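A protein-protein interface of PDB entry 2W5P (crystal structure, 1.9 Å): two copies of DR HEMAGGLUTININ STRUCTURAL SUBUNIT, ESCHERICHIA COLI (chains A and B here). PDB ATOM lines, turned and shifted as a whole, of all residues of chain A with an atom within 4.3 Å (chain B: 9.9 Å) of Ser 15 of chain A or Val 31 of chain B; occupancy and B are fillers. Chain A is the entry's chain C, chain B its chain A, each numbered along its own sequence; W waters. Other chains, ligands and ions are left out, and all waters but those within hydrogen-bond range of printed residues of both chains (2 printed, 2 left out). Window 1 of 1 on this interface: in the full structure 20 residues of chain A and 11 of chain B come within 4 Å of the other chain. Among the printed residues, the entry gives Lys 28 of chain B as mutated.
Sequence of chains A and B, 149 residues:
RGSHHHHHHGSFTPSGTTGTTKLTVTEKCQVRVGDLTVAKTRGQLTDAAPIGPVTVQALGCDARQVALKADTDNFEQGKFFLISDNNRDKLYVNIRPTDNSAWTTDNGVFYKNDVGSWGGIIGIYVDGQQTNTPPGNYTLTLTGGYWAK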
ATOM      1  N   THR A  13       4.469 -28.082 -15.226  1.00  0.00           N
ATOM      2  CA  THR A  13       4.092 -28.453 -16.581  1.00  0.00           C
ATOM      3  C   THR A  13       4.558 -27.336 -17.498  1.00  0.00           C
ATOM      4  O   THR A  13       4.029 -26.252 -17.438  1.00  0.00           O
ATOM      5  CB  THR A  13       2.567 -28.658 -16.713  1.00  0.00           C
ATOM      6  OG1 THR A  13       2.156 -29.735 -15.862  1.00  0.00           O
ATOM      7  CG2 THR A  13       2.184 -28.981 -18.192  1.00  0.00           C
ATOM      8  N   PRO A  14       5.519 -27.613 -18.371  1.00  0.00           N
ATOM      9  CA  PRO A  14       5.965 -26.574 -19.308  1.00  0.00           C
ATOM     10  C   PRO A  14       4.815 -26.218 -20.268  1.00  0.00           C
ATOM     11  O   PRO A  14       4.217 -27.095 -20.895  1.00  0.00           O
ATOM     12  CB  PRO A  14       7.144 -27.218 -20.064  1.00  0.00           C
ATOM     13  CG  PRO A  14       7.487 -28.474 -19.312  1.00  0.00           C
ATOM     14  CD  PRO A  14       6.350 -28.840 -18.417  1.00  0.00           C
ATOM     15  N   SER A  15       4.479 -24.932 -20.334  1.00  0.00           N
ATOM     16  CA  SER A  15       3.379 -24.491 -21.193  1.00  0.00           C
ATOM     17  C   SER A  15       3.391 -22.992 -21.439  1.00  0.00           C
ATOM     18  O   SER A  15       2.754 -22.239 -20.732  1.00  0.00           O
ATOM     19  CB  SER A  15       2.021 -24.936 -20.655  1.00  0.00           C
ATOM     20  OG  SER A  15       1.019 -24.576 -21.609  1.00  0.00           O
ATOM     21  N   GLY A  16       4.183 -22.575 -22.436  1.00  0.00           N
ATOM     22  CA  GLY A  16       4.393 -21.169 -22.733  1.00  0.00           C
ATOM     23  C   GLY A  16       5.803 -20.964 -23.271  1.00  0.00           C
ATOM     24  O   GLY A  16       6.502 -21.917 -23.625  1.00  0.00           O
ATOM     25  N   THR A  17       6.210 -19.711 -23.347  1.00  0.00           N
ATOM     26  CA  THR A  17       7.470 -19.374 -23.976  1.00  0.00           C
ATOM     27  C   THR A  17       8.640 -19.267 -23.028  1.00  0.00           C
ATOM     28  O   THR A  17       8.470 -19.172 -21.815  1.00  0.00           O
ATOM     29  CB  THR A  17       7.327 -18.106 -24.850  1.00  0.00           C
ATOM     30  OG1 THR A  17       6.902 -17.025 -24.019  1.00  0.00           O
ATOM     31  CG2 THR A  17       6.266 -18.345 -25.926  1.00  0.00           C
ATOM     32  N   VAL A  56       5.938 -11.090 -17.947  1.00  0.00           N
ATOM     33  CA  VAL A  56       5.187 -12.349 -17.899  1.00  0.00           C
ATOM     34  C   VAL A  56       3.722 -12.056 -18.162  1.00  0.00           C
ATOM     35  O   VAL A  56       3.153 -11.173 -17.544  1.00  0.00           O
ATOM     36  CB  VAL A  56       5.347 -13.069 -16.526  1.00  0.00           C
ATOM     37  CG1 VAL A  56       4.445 -14.362 -16.462  1.00  0.00           C
ATOM     38  CG2 VAL A  56       6.834 -13.406 -16.232  1.00  0.00           C
ATOM     39  N   GLN A  57       3.095 -12.863 -19.014  1.00  0.00           N
ATOM     40  CA  GLN A  57       1.657 -12.754 -19.250  1.00  0.00           C
ATOM     41  C   GLN A  57       1.060 -14.145 -19.450  1.00  0.00           C
ATOM     42  O   GLN A  57       1.321 -14.808 -20.454  1.00  0.00           O
ATOM     43  CB  GLN A  57       1.338 -11.865 -20.488  1.00  0.00           C
ATOM     44  CG  GLN A  57      -0.168 -11.658 -20.687  1.00  0.00           C
ATOM     45  CD  GLN A  57      -0.805 -10.985 -19.487  1.00  0.00           C
ATOM     46  OE1 GLN A  57      -0.418  -9.871 -19.138  1.00  0.00           O
ATOM     47  NE2 GLN A  57      -1.736 -11.699 -18.785  1.00  0.00           N
ATOM     48  N   ALA A  58       0.219 -14.555 -18.511  1.00  0.00           N
ATOM     49  CA  ALA A  58      -0.515 -15.817 -18.623  1.00  0.00           C
ATOM     50  C   ALA A  58      -1.867 -15.603 -19.286  1.00  0.00           C
ATOM     51  O   ALA A  58      -2.488 -14.531 -19.153  1.00  0.00           O
ATOM     52  CB  ALA A  58      -0.712 -16.437 -17.243  1.00  0.00           C
ATOM     53  N   CYS A  61      -5.288 -19.505 -17.773  1.00  0.00           N
ATOM     54  CA  CYS A  61      -4.869 -20.142 -16.539  1.00  0.00           C
ATOM     55  C   CYS A  61      -5.760 -19.715 -15.390  1.00  0.00           C
ATOM     56  O   CYS A  61      -5.291 -19.635 -14.275  1.00  0.00           O
ATOM     57  CB  CYS A  61      -3.437 -19.696 -16.210  1.00  0.00           C
ATOM     58  SG  CYS A  61      -2.239 -20.038 -17.516  1.00  0.00           S
ATOM     59  N   VAL A  66       0.220 -20.117 -12.156  1.00  0.00           N
ATOM     60  CA  VAL A  66       1.263 -19.716 -13.105  1.00  0.00           C
ATOM     61  C   VAL A  66       2.624 -20.011 -12.491  1.00  0.00           C
ATOM     62  O   VAL A  66       2.833 -19.821 -11.299  1.00  0.00           O
ATOM     63  CB  VAL A  66       1.132 -18.218 -13.490  1.00  0.00           C
ATOM     64  CG1 VAL A  66       2.441 -17.730 -14.142  1.00  0.00           C
ATOM     65  CG2 VAL A  66      -0.119 -18.002 -14.429  1.00  0.00           C
ATOM     66  N   ALA A  67       3.560 -20.436 -13.312  1.00  0.00           N
ATOM     67  CA  ALA A  67       4.920 -20.727 -12.846  1.00  0.00           C
ATOM     68  C   ALA A  67       5.956 -20.465 -13.924  1.00  0.00           C
ATOM     69  O   ALA A  67       5.638 -20.429 -15.110  1.00  0.00           O
ATOM     70  CB  ALA A  67       5.034 -22.180 -12.387  1.00  0.00           C
ATOM     71  N   GLY A 144       7.926 -20.547 -19.244  1.00  0.00           N
ATOM     72  CA  GLY A 144       6.588 -20.442 -18.671  1.00  0.00           C
ATOM     73  C   GLY A 144       5.829 -21.797 -18.612  1.00  0.00           C
ATOM     74  O   GLY A 144       6.043 -22.678 -19.423  1.00  0.00           O
ATOM     75  N   GLY A 145       4.924 -21.938 -17.644  1.00  0.00           N
ATOM     76  CA  GLY A 145       4.123 -23.148 -17.548  1.00  0.00           C
ATOM     77  C   GLY A 145       3.299 -23.042 -16.288  1.00  0.00           C
ATOM     78  O   GLY A 145       3.059 -21.950 -15.802  1.00  0.00           O
ATOM     79  N   TYR A 146       2.857 -24.177 -15.761  1.00  0.00           N
ATOM     80  CA  TYR A 146       2.050 -24.143 -14.546  1.00  0.00           C
ATOM     81  C   TYR A 146       2.407 -25.216 -13.536  1.00  0.00           C
ATOM     82  O   TYR A 146       3.053 -26.214 -13.866  1.00  0.00           O
ATOM     83  CB  TYR A 146       0.547 -24.078 -14.832  1.00  0.00           C
ATOM     84  CG  TYR A 146       0.005 -25.225 -15.665  1.00  0.00           C
ATOM     85  CD1 TYR A 146      -0.097 -25.113 -17.048  1.00  0.00           C
ATOM     86  CD2 TYR A 146      -0.429 -26.406 -15.071  1.00  0.00           C
ATOM     87  CE1 TYR A 146      -0.581 -26.157 -17.826  1.00  0.00           C
ATOM     88  CE2 TYR A 146      -0.928 -27.477 -15.866  1.00  0.00           C
ATOM     89  CZ  TYR A 146      -0.992 -27.328 -17.230  1.00  0.00           C
ATOM     90  OH  TYR A 146      -1.476 -28.355 -18.017  1.00  0.00           O
ATOM     91  N   THR B  24       5.685 -21.763 -30.638  1.00  0.00           N
ATOM     92  CA  THR B  24       5.695 -22.475 -29.370  1.00  0.00           C
ATOM     93  C   THR B  24       4.310 -23.100 -29.209  1.00  0.00           C
ATOM     94  O   THR B  24       3.314 -22.399 -29.276  1.00  0.00           O
ATOM     95  CB  THR B  24       6.072 -21.596 -28.150  1.00  0.00           C
ATOM     96  OG1 THR B  24       7.405 -21.088 -28.304  1.00  0.00           O
ATOM     97  CG2 THR B  24       6.007 -22.458 -26.865  1.00  0.00           C
ATOM     98  N   VAL B  25       4.253 -24.425 -29.065  1.00  0.00           N
ATOM     99  CA  VAL B  25       2.965 -25.125 -28.882  1.00  0.00           C
ATOM    100  C   VAL B  25       2.804 -25.310 -27.381  1.00  0.00           C
ATOM    101  O   VAL B  25       3.743 -25.744 -26.701  1.00  0.00           O
ATOM    102  CB  VAL B  25       2.940 -26.506 -29.614  1.00  0.00           C
ATOM    103  CG1 VAL B  25       1.584 -27.249 -29.331  1.00  0.00           C
ATOM    104  CG2 VAL B  25       3.137 -26.321 -31.106  1.00  0.00           C
ATOM    105  N   THR B  26       1.632 -24.936 -26.861  1.00  0.00           N
ATOM    106  CA  THR B  26       1.385 -24.953 -25.421  1.00  0.00           C
ATOM    107  C   THR B  26       0.111 -25.705 -25.073  1.00  0.00           C
ATOM    108  O   THR B  26      -0.632 -26.103 -25.953  1.00  0.00           O
ATOM    109  CB  THR B  26       1.245 -23.488 -24.900  1.00  0.00           C
ATOM    110  OG1 THR B  26      -0.021 -22.936 -25.317  1.00  0.00           O
ATOM    111  CG2 THR B  26       2.359 -22.622 -25.447  1.00  0.00           C
ATOM    112  N   GLU B  27      -0.170 -25.833 -23.774  1.00  0.00           N
ATOM    113  CA  GLU B  27      -1.480 -26.323 -23.325  1.00  0.00           C
ATOM    114  C   GLU B  27      -2.423 -25.108 -23.282  1.00  0.00           C
ATOM    115  O   GLU B  27      -2.028 -23.970 -23.639  1.00  0.00           O
ATOM    116  CB  GLU B  27      -1.372 -26.936 -21.931  1.00  0.00           C
ATOM    117  CG  GLU B  27      -0.414 -28.117 -21.856  1.00  0.00           C
ATOM    118  CD  GLU B  27      -0.942 -29.346 -22.564  1.00  0.00           C
ATOM    119  OE1 GLU B  27      -0.185 -30.325 -22.699  1.00  0.00           O
ATOM    120  OE2 GLU B  27      -2.121 -29.349 -22.960  1.00  0.00           O
ATOM    121  N   LYS B  28      -3.634 -25.310 -22.771  1.00  0.00           N
ATOM    122  CA  LYS B  28      -4.586 -24.209 -22.697  1.00  0.00           C
ATOM    123  C   LYS B  28      -4.098 -23.058 -21.829  1.00  0.00           C
ATOM    124  O   LYS B  28      -4.263 -21.909 -22.183  1.00  0.00           O
ATOM    125  CB  LYS B  28      -5.974 -24.683 -22.233  1.00  0.00           C
ATOM    126  CG  LYS B  28      -7.057 -23.617 -22.408  1.00  0.00           C
ATOM    127  CD  LYS B  28      -7.749 -23.281 -21.082  1.00  0.00           C
ATOM    128  CE  LYS B  28      -8.738 -22.122 -21.245  1.00  0.00           C
ATOM    129  NZ  LYS B  28      -8.572 -21.413 -22.561  1.00  0.00           N
ATOM    130  N   CYS B  29      -3.556 -23.386 -20.661  1.00  0.00           N
ATOM    131  CA  CYS B  29      -2.974 -22.394 -19.770  1.00  0.00           C
ATOM    132  C   CYS B  29      -1.568 -22.158 -20.349  1.00  0.00           C
ATOM    133  O   CYS B  29      -0.732 -23.083 -20.439  1.00  0.00           O
ATOM    134  CB  CYS B  29      -2.880 -22.943 -18.348  1.00  0.00           C
ATOM    135  SG  CYS B  29      -1.834 -22.000 -17.216  1.00  0.00           S
ATOM    136  N   GLN B  30      -1.383 -20.938 -20.821  1.00  0.00           N
ATOM    137  CA  GLN B  30      -0.248 -20.529 -21.629  1.00  0.00           C
ATOM    138  C   GLN B  30       0.425 -19.371 -20.924  1.00  0.00           C
ATOM    139  O   GLN B  30      -0.219 -18.374 -20.650  1.00  0.00           O
ATOM    140  CB  GLN B  30      -0.810 -20.064 -22.991  1.00  0.00           C
ATOM    141  CG  GLN B  30       0.210 -19.745 -24.064  1.00  0.00           C
ATOM    142  CD  GLN B  30      -0.458 -19.208 -25.311  1.00  0.00           C
ATOM    143  OE1 GLN B  30      -0.750 -18.010 -25.394  1.00  0.00           O
ATOM    144  NE2 GLN B  30      -0.848 -20.112 -26.219  1.00  0.00           N
ATOM    145  N   VAL B  31       1.712 -19.537 -20.589  1.00  0.00           N
ATOM    146  CA  VAL B  31       2.490 -18.497 -19.877  1.00  0.00           C
ATOM    147  C   VAL B  31       3.613 -17.914 -20.752  1.00  0.00           C
ATOM    148  O   VAL B  31       4.647 -18.553 -20.991  1.00  0.00           O
ATOM    149  CB  VAL B  31       2.980 -19.004 -18.513  1.00  0.00           C
ATOM    150  CG1 VAL B  31       3.774 -17.911 -17.784  1.00  0.00           C
ATOM    151  CG2 VAL B  31       1.731 -19.439 -17.654  1.00  0.00           C
ATOM    152  N   ARG B  32       3.362 -16.724 -21.272  1.00  0.00           N
ATOM    153  CA  ARG B  32       4.298 -16.043 -22.150  1.00  0.00           C
ATOM    154  C   ARG B  32       5.344 -15.316 -21.287  1.00  0.00           C
ATOM    155  O   ARG B  32       4.980 -14.591 -20.378  1.00  0.00           O
ATOM    156  CB  ARG B  32       3.515 -15.051 -23.010  1.00  0.00           C
ATOM    157  CG  ARG B  32       2.728 -15.744 -24.124  1.00  0.00           C
ATOM    158  CD  ARG B  32       1.528 -14.943 -24.607  1.00  0.00           C
ATOM    159  NE  ARG B  32       0.736 -15.678 -25.608  1.00  0.00           N
ATOM    160  CZ  ARG B  32       1.061 -15.791 -26.895  1.00  0.00           C
ATOM    161  NH1 ARG B  32       2.174 -15.242 -27.358  1.00  0.00           N
ATOM    162  NH2 ARG B  32       0.266 -16.448 -27.730  1.00  0.00           N
ATOM    163  N   VAL B  33       6.628 -15.629 -21.521  1.00  0.00           N
ATOM    164  CA  VAL B  33       7.746 -15.048 -20.798  1.00  0.00           C
ATOM    165  C   VAL B  33       8.643 -14.311 -21.805  1.00  0.00           C
ATOM    166  O   VAL B  33       9.104 -14.897 -22.788  1.00  0.00           O
ATOM    167  CB  VAL B  33       8.600 -16.184 -20.078  1.00  0.00           C
ATOM    168  CG1 VAL B  33       9.730 -15.547 -19.230  1.00  0.00           C
ATOM    169  CG2 VAL B  33       7.699 -17.065 -19.212  1.00  0.00           C
ATOM    170  N   GLY B  34       8.947 -13.059 -21.506  1.00  0.00           N
ATOM    171  CA  GLY B  34       9.815 -12.269 -22.350  1.00  0.00           C
ATOM    172  C   GLY B  34       9.072 -11.712 -23.574  1.00  0.00           C
ATOM    173  O   GLY B  34       7.836 -11.642 -23.608  1.00  0.00           O
ATOM    174  N   ASP B  35       9.826 -11.319 -24.592  1.00  0.00           N
ATOM    175  CA  ASP B  35       9.191 -10.681 -25.724  1.00  0.00           C
ATOM    176  C   ASP B  35       8.266 -11.552 -26.538  1.00  0.00           C
ATOM    177  O   ASP B  35       8.379 -12.786 -26.553  1.00  0.00           O
ATOM    178  CB  ASP B  35      10.146  -9.849 -26.581  1.00  0.00           C
ATOM    179  CG  ASP B  35      11.446 -10.536 -26.842  1.00  0.00           C
ATOM    180  OD1 ASP B  35      12.504  -9.908 -26.607  1.00  0.00           O
ATOM    181  OD2 ASP B  35      11.414 -11.642 -27.425  1.00  0.00           O
ATOM    182  N   THR B  37       6.248 -13.636 -29.091  1.00  0.00           N
ATOM    183  CA  THR B  37       6.603 -14.616 -30.114  1.00  0.00           C
ATOM    184  C   THR B  37       5.307 -15.375 -30.413  1.00  0.00           C
ATOM    185  O   THR B  37       4.333 -15.266 -29.657  1.00  0.00           O
ATOM    186  CB  THR B  37       7.722 -15.574 -29.647  1.00  0.00           C
ATOM    187  OG1 THR B  37       7.244 -16.387 -28.570  1.00  0.00           O
ATOM    188  CG2 THR B  37       8.976 -14.784 -29.182  1.00  0.00           C
ATOM    189  N   ALA B  39       2.811 -18.222 -30.400  1.00  0.00           N
ATOM    190  CA  ALA B  39       2.497 -19.393 -29.602  1.00  0.00           C
ATOM    191  C   ALA B  39       1.064 -19.776 -29.950  1.00  0.00           C
ATOM    192  O   ALA B  39       0.221 -18.916 -30.248  1.00  0.00           O
ATOM    193  CB  ALA B  39       2.631 -19.082 -28.111  1.00  0.00           C
ATOM    194  N   LYS B  40       0.801 -21.071 -29.942  1.00  0.00           N
ATOM    195  CA  LYS B  40      -0.547 -21.566 -30.200  1.00  0.00           C
ATOM    196  C   LYS B  40      -0.809 -22.758 -29.301  1.00  0.00           C
ATOM    197  O   LYS B  40       0.120 -23.504 -28.985  1.00  0.00           O
ATOM    198  CB  LYS B  40      -0.696 -21.918 -31.692  1.00  0.00           C
ATOM    199  CG  LYS B  40      -1.578 -20.879 -32.437  1.00  0.00           C
ATOM    200  CD  LYS B  40      -1.084 -20.567 -33.819  1.00  0.00           C
ATOM    201  CE  LYS B  40      -1.203 -19.053 -34.138  1.00  0.00           C
ATOM    202  NZ  LYS B  40      -2.608 -18.598 -34.298  1.00  0.00           N
ATOM    203  N   THR B  41      -2.033 -22.894 -28.779  1.00  0.00           N
ATOM    204  CA  THR B  41      -2.294 -24.057 -27.910  1.00  0.00           C
ATOM    205  C   THR B  41      -2.386 -25.253 -28.865  1.00  0.00           C
ATOM    206  O   THR B  41      -2.626 -25.074 -30.060  1.00  0.00           O
ATOM    207  CB  THR B  41      -3.615 -23.925 -27.087  1.00  0.00           C
ATOM    208  OG1 THR B  41      -4.729 -23.981 -27.978  1.00  0.00           O
ATOM    209  CG2 THR B  41      -3.644 -22.633 -26.267  1.00  0.00           C
ATOM    210  N   ARG B  42      -2.214 -26.463 -28.355  1.00  0.00           N
ATOM    211  CA  ARG B  42      -2.341 -27.618 -29.223  1.00  0.00           C
ATOM    212  C   ARG B  42      -3.771 -27.791 -29.770  1.00  0.00           C
ATOM    213  O   ARG B  42      -3.959 -28.290 -30.885  1.00  0.00           O
ATOM    214  CB  ARG B  42      -1.818 -28.892 -28.560  1.00  0.00           C
ATOM    215  CG  ARG B  42      -2.355 -29.133 -27.197  1.00  0.00           C
ATOM    216  CD  ARG B  42      -1.492 -30.137 -26.478  1.00  0.00           C
ATOM    217  NE  ARG B  42      -2.267 -30.915 -25.521  1.00  0.00           N
ATOM    218  CZ  ARG B  42      -1.833 -32.034 -24.955  1.00  0.00           C
ATOM    219  NH1 ARG B  42      -0.619 -32.501 -25.243  1.00  0.00           N
ATOM    220  NH2 ARG B  42      -2.606 -32.678 -24.093  1.00  0.00           N
ATOM    221  N   GLY B  43      -4.761 -27.309 -29.018  1.00  0.00           N
ATOM    222  CA  GLY B  43      -6.148 -27.365 -29.463  1.00  0.00           C
ATOM    223  C   GLY B  43      -6.375 -26.476 -30.689  1.00  0.00           C
ATOM    224  O   GLY B  43      -7.360 -26.644 -31.415  1.00  0.00           O
ATOM    225  N   THR B 133      -0.108 -32.562 -30.990  1.00  0.00           N
ATOM    226  CA  THR B 133       1.275 -32.046 -31.024  1.00  0.00           C
ATOM    227  C   THR B 133       1.804 -31.774 -29.612  1.00  0.00           C
ATOM    228  O   THR B 133       1.186 -31.056 -28.833  1.00  0.00           O
ATOM    229  CB  THR B 133       1.411 -30.773 -31.927  1.00  0.00           C
ATOM    230  OG1 THR B 133       1.008 -31.082 -33.265  1.00  0.00           O
ATOM    231  CG2 THR B 133       2.869 -30.287 -31.944  1.00  0.00           C
ATOM    232  N   PRO B 134       2.943 -32.367 -29.272  1.00  0.00           N
ATOM    233  CA  PRO B 134       3.490 -32.191 -27.939  1.00  0.00           C
ATOM    234  C   PRO B 134       3.927 -30.742 -27.771  1.00  0.00           C
ATOM    235  O   PRO B 134       4.480 -30.144 -28.704  1.00  0.00           O
ATOM    236  CB  PRO B 134       4.719 -33.121 -27.947  1.00  0.00           C
ATOM    237  CG  PRO B 134       4.391 -34.158 -28.928  1.00  0.00           C
ATOM    238  CD  PRO B 134       3.599 -33.476 -29.998  1.00  0.00           C
ATOM    239  N   PRO B 135       3.645 -30.168 -26.611  1.00  0.00           N
ATOM    240  CA  PRO B 135       4.068 -28.795 -26.341  1.00  0.00           C
ATOM    241  C   PRO B 135       5.589 -28.766 -26.550  1.00  0.00           C
ATOM    242  O   PRO B 135       6.298 -29.735 -26.228  1.00  0.00           O
ATOM    243  CB  PRO B 135       3.744 -28.625 -24.846  1.00  0.00           C
ATOM    244  CG  PRO B 135       2.574 -29.530 -24.628  1.00  0.00           C
ATOM    245  CD  PRO B 135       2.866 -30.732 -25.491  1.00  0.00           C
ATOM    246  N   GLY B 136       6.083 -27.656 -27.066  1.00  0.00           N
ATOM    247  CA  GLY B 136       7.522 -27.498 -27.287  1.00  0.00           C
ATOM    248  C   GLY B 136       7.759 -26.366 -28.267  1.00  0.00           C
ATOM    249  O   GLY B 136       6.854 -25.598 -28.543  1.00  0.00           O
ATOM    250  N   ASN B 137       9.004 -26.219 -28.714  1.00  0.00           N
ATOM    251  CA  ASN B 137       9.364 -25.135 -29.636  1.00  0.00           C
ATOM    252  C   ASN B 137       9.683 -25.723 -30.989  1.00  0.00           C
ATOM    253  O   ASN B 137      10.392 -26.734 -31.108  1.00  0.00           O
ATOM    254  CB  ASN B 137      10.519 -24.271 -29.084  1.00  0.00           C
ATOM    255  CG  ASN B 137      10.092 -23.462 -27.872  1.00  0.00           C
ATOM    256  OD1 ASN B 137       9.389 -22.472 -27.997  1.00  0.00           O
ATOM    257  ND2 ASN B 137      10.466 -23.924 -26.689  1.00  0.00           N
HETATM  258  O   HOH W   1      -3.722 -26.175 -19.373  1.00  0.00           O
HETATM  259  O   HOH W   2       9.373 -22.764 -24.335  1.00  0.00           O
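Of the 14 printed residues of chain A, 11 touch a printed residue of chain B. Of the 23 printed residues of chain B, 9 touch a printed residue of chain A. Hydrophobic or aromatic side chains of chain B that line the printed part of chain A: Val 31 and Val 33. Among the printed residues, no Asp or Glu carboxylate lies within 4 Å of a Lys or Arg side-chain nitrogen of the other chain.
The backbone carbonyl oxygen (O) of Thr 24 of chain B is in hydrogen-bond range of the backbone NH (N) of Lys 40 of chain B, 2.9 Å away. The side-chain hydroxyl of Thr 24 of chain B lies within hydrogen-bond range of the side-chain amide oxygen of Asn 137 of chain B. O of Lys 40 of chain B lies within hydrogen-bond range of N of Thr 26 of chain B, at 3.0 Å. The guanidinium group (NE) of Arg 42 of chain B is in salt-bridge range of the side-chain carboxylate (OE2) of Glu 27 of chain B, 3.0 Å away. The side-chain amide oxygen (OE1) of Gln 30 of chain B lies within hydrogen-bond range of the guanidinium group (NE) of Arg 32 of chain B, 2.8 Å away. O of Gly 144 of chain A sits at hydrogen-bond distance from N of Ser 15 of chain A, at 2.9 Å.
The backbone NH (N) of Glu 27 of chain B sits at hydrogen-bond distance from the side-chain hydroxyl (OG) of Ser 15 of chain A (2.8 Å). O of Cys 29 of chain B is in hydrogen-bond range of OG of Ser 15 of chain A (2.6 Å). The side-chain sulfur (SG) of Cys 29 of chain B is disulfide-bonded to the side-chain sulfur (SG) of Cys 61 of chain A, at 2.0 Å. The side-chain sulfur (SG) of Cys 61 of chain A sits at hydrogen-bond distance from the backbone NH (N) of Gln 30 of chain B, 3.5 Å away. The backbone NH (N) of Val 31 of chain B lies within hydrogen-bond range of the backbone carbonyl oxygen (O) of Ser 15 of chain A (2.9 Å). The backbone NH of Thr 17 of chain A sits at hydrogen-bond distance from the backbone carbonyl oxygen of Val 31 of chain B (3.1 Å). O of Arg 32 of chain B sits at hydrogen-bond distance from N of Gln 57 of chain A (2.9 Å). The backbone NH (N) of Val 33 of chain B sits at hydrogen-bond distance from the side-chain hydroxyl (OG1) of Thr 17 of chain A (2.9 Å).
Water W2 bridges the side-chain amide nitrogen of Asn 137 of chain B (2.8 Å) and the backbone carbonyl oxygen of Gly 16 of chain A (3.1 Å). Water W1 lies within hydrogen-bond range of N of Cys 29 of chain B (3.1 Å) and OH of Tyr 146 of chain A (3.4 Å).
Among the printed residues, merely in contact across the chains: Gly 16 of chain A with Val 31 of chain B (3.2 Å), Ala 58 of chain A with Gln 30 of chain B (3.3 Å), Gly 16 of chain A with Thr 24 of chain B (3.3 Å), Val 56 of chain A with Arg 32 of chain B (3.3 Å), Thr 17 of chain A with Arg 32 of chain B (3.4 Å), Gly 145 of chain A with Val 31 of chain B (3.4 Å), Thr 17 of chain A with Thr 37 of chain B (3.4 Å), Ser 15 of chain A with Thr 26 of chain B (3.5 Å), Gly 144 of chain A with Val 33 of chain B (3.5 Å), Gly 16 of chain A with Thr 26 of chain B (3.5 Å), Gly 144 of chain A with Val 31 of chain B (3.6 Å), Tyr 146 of chain A with Cys 29 of chain B (3.6 Å), Ser 15 of chain A with Gln 30 of chain B (3.6 Å), Thr 17 of chain A with Thr 24 of chain B (3.8 Å), Val 56 of chain A with Val 31 of chain B (3.8 Å), Gln 57 of chain A with Val 31 of chain B (3.9 Å), Val 66 of chain A with Val 31 of chain B (3.9 Å), Gln 57 of chain A with Gln 30 of chain B (3.9 Å), Ala 58 of chain A with Val 31 of chain B (3.9 Å) and Tyr 146 of chain A with Glu 27 of chain B (3.99 Å).
Ser 15 of chain A touches five residues of chain B. Of the printed residues of chain A, Val 31 of chain B touches Ser 15 (2.9 Å), Gly 16 (3.2 Å), Thr 17 (3.1 Å), Val 56 (3.8 Å), Gln 57 (3.9 Å), Ala 58 (3.9 Å), Val 66 (3.9 Å), Gly 144 (3.6 Å) and Gly 145 (3.4 Å). No residue of chain B comes within 4 Å of Pro 14 of chain A. Of the printed residues of chain A, Thr 26 of chain B touches Ser 15 and Gly 16. Printed residues of chain A within 4 Å of Glu 27 of chain B: Ser 15 and Tyr 146. The nearest residue of chain B that does not touch Ser 15 of chain A is Lys 28 of chain B (4.9 Å). The nearest printed residue of chain A that does not touch Val 31 of chain B is Cys 61 of chain A (4.02 Å). The nearest printed residue of chain A that does not touch Val 33 of chain B is Val 56 of chain A (4.7 Å).
No position is printed for both chains.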
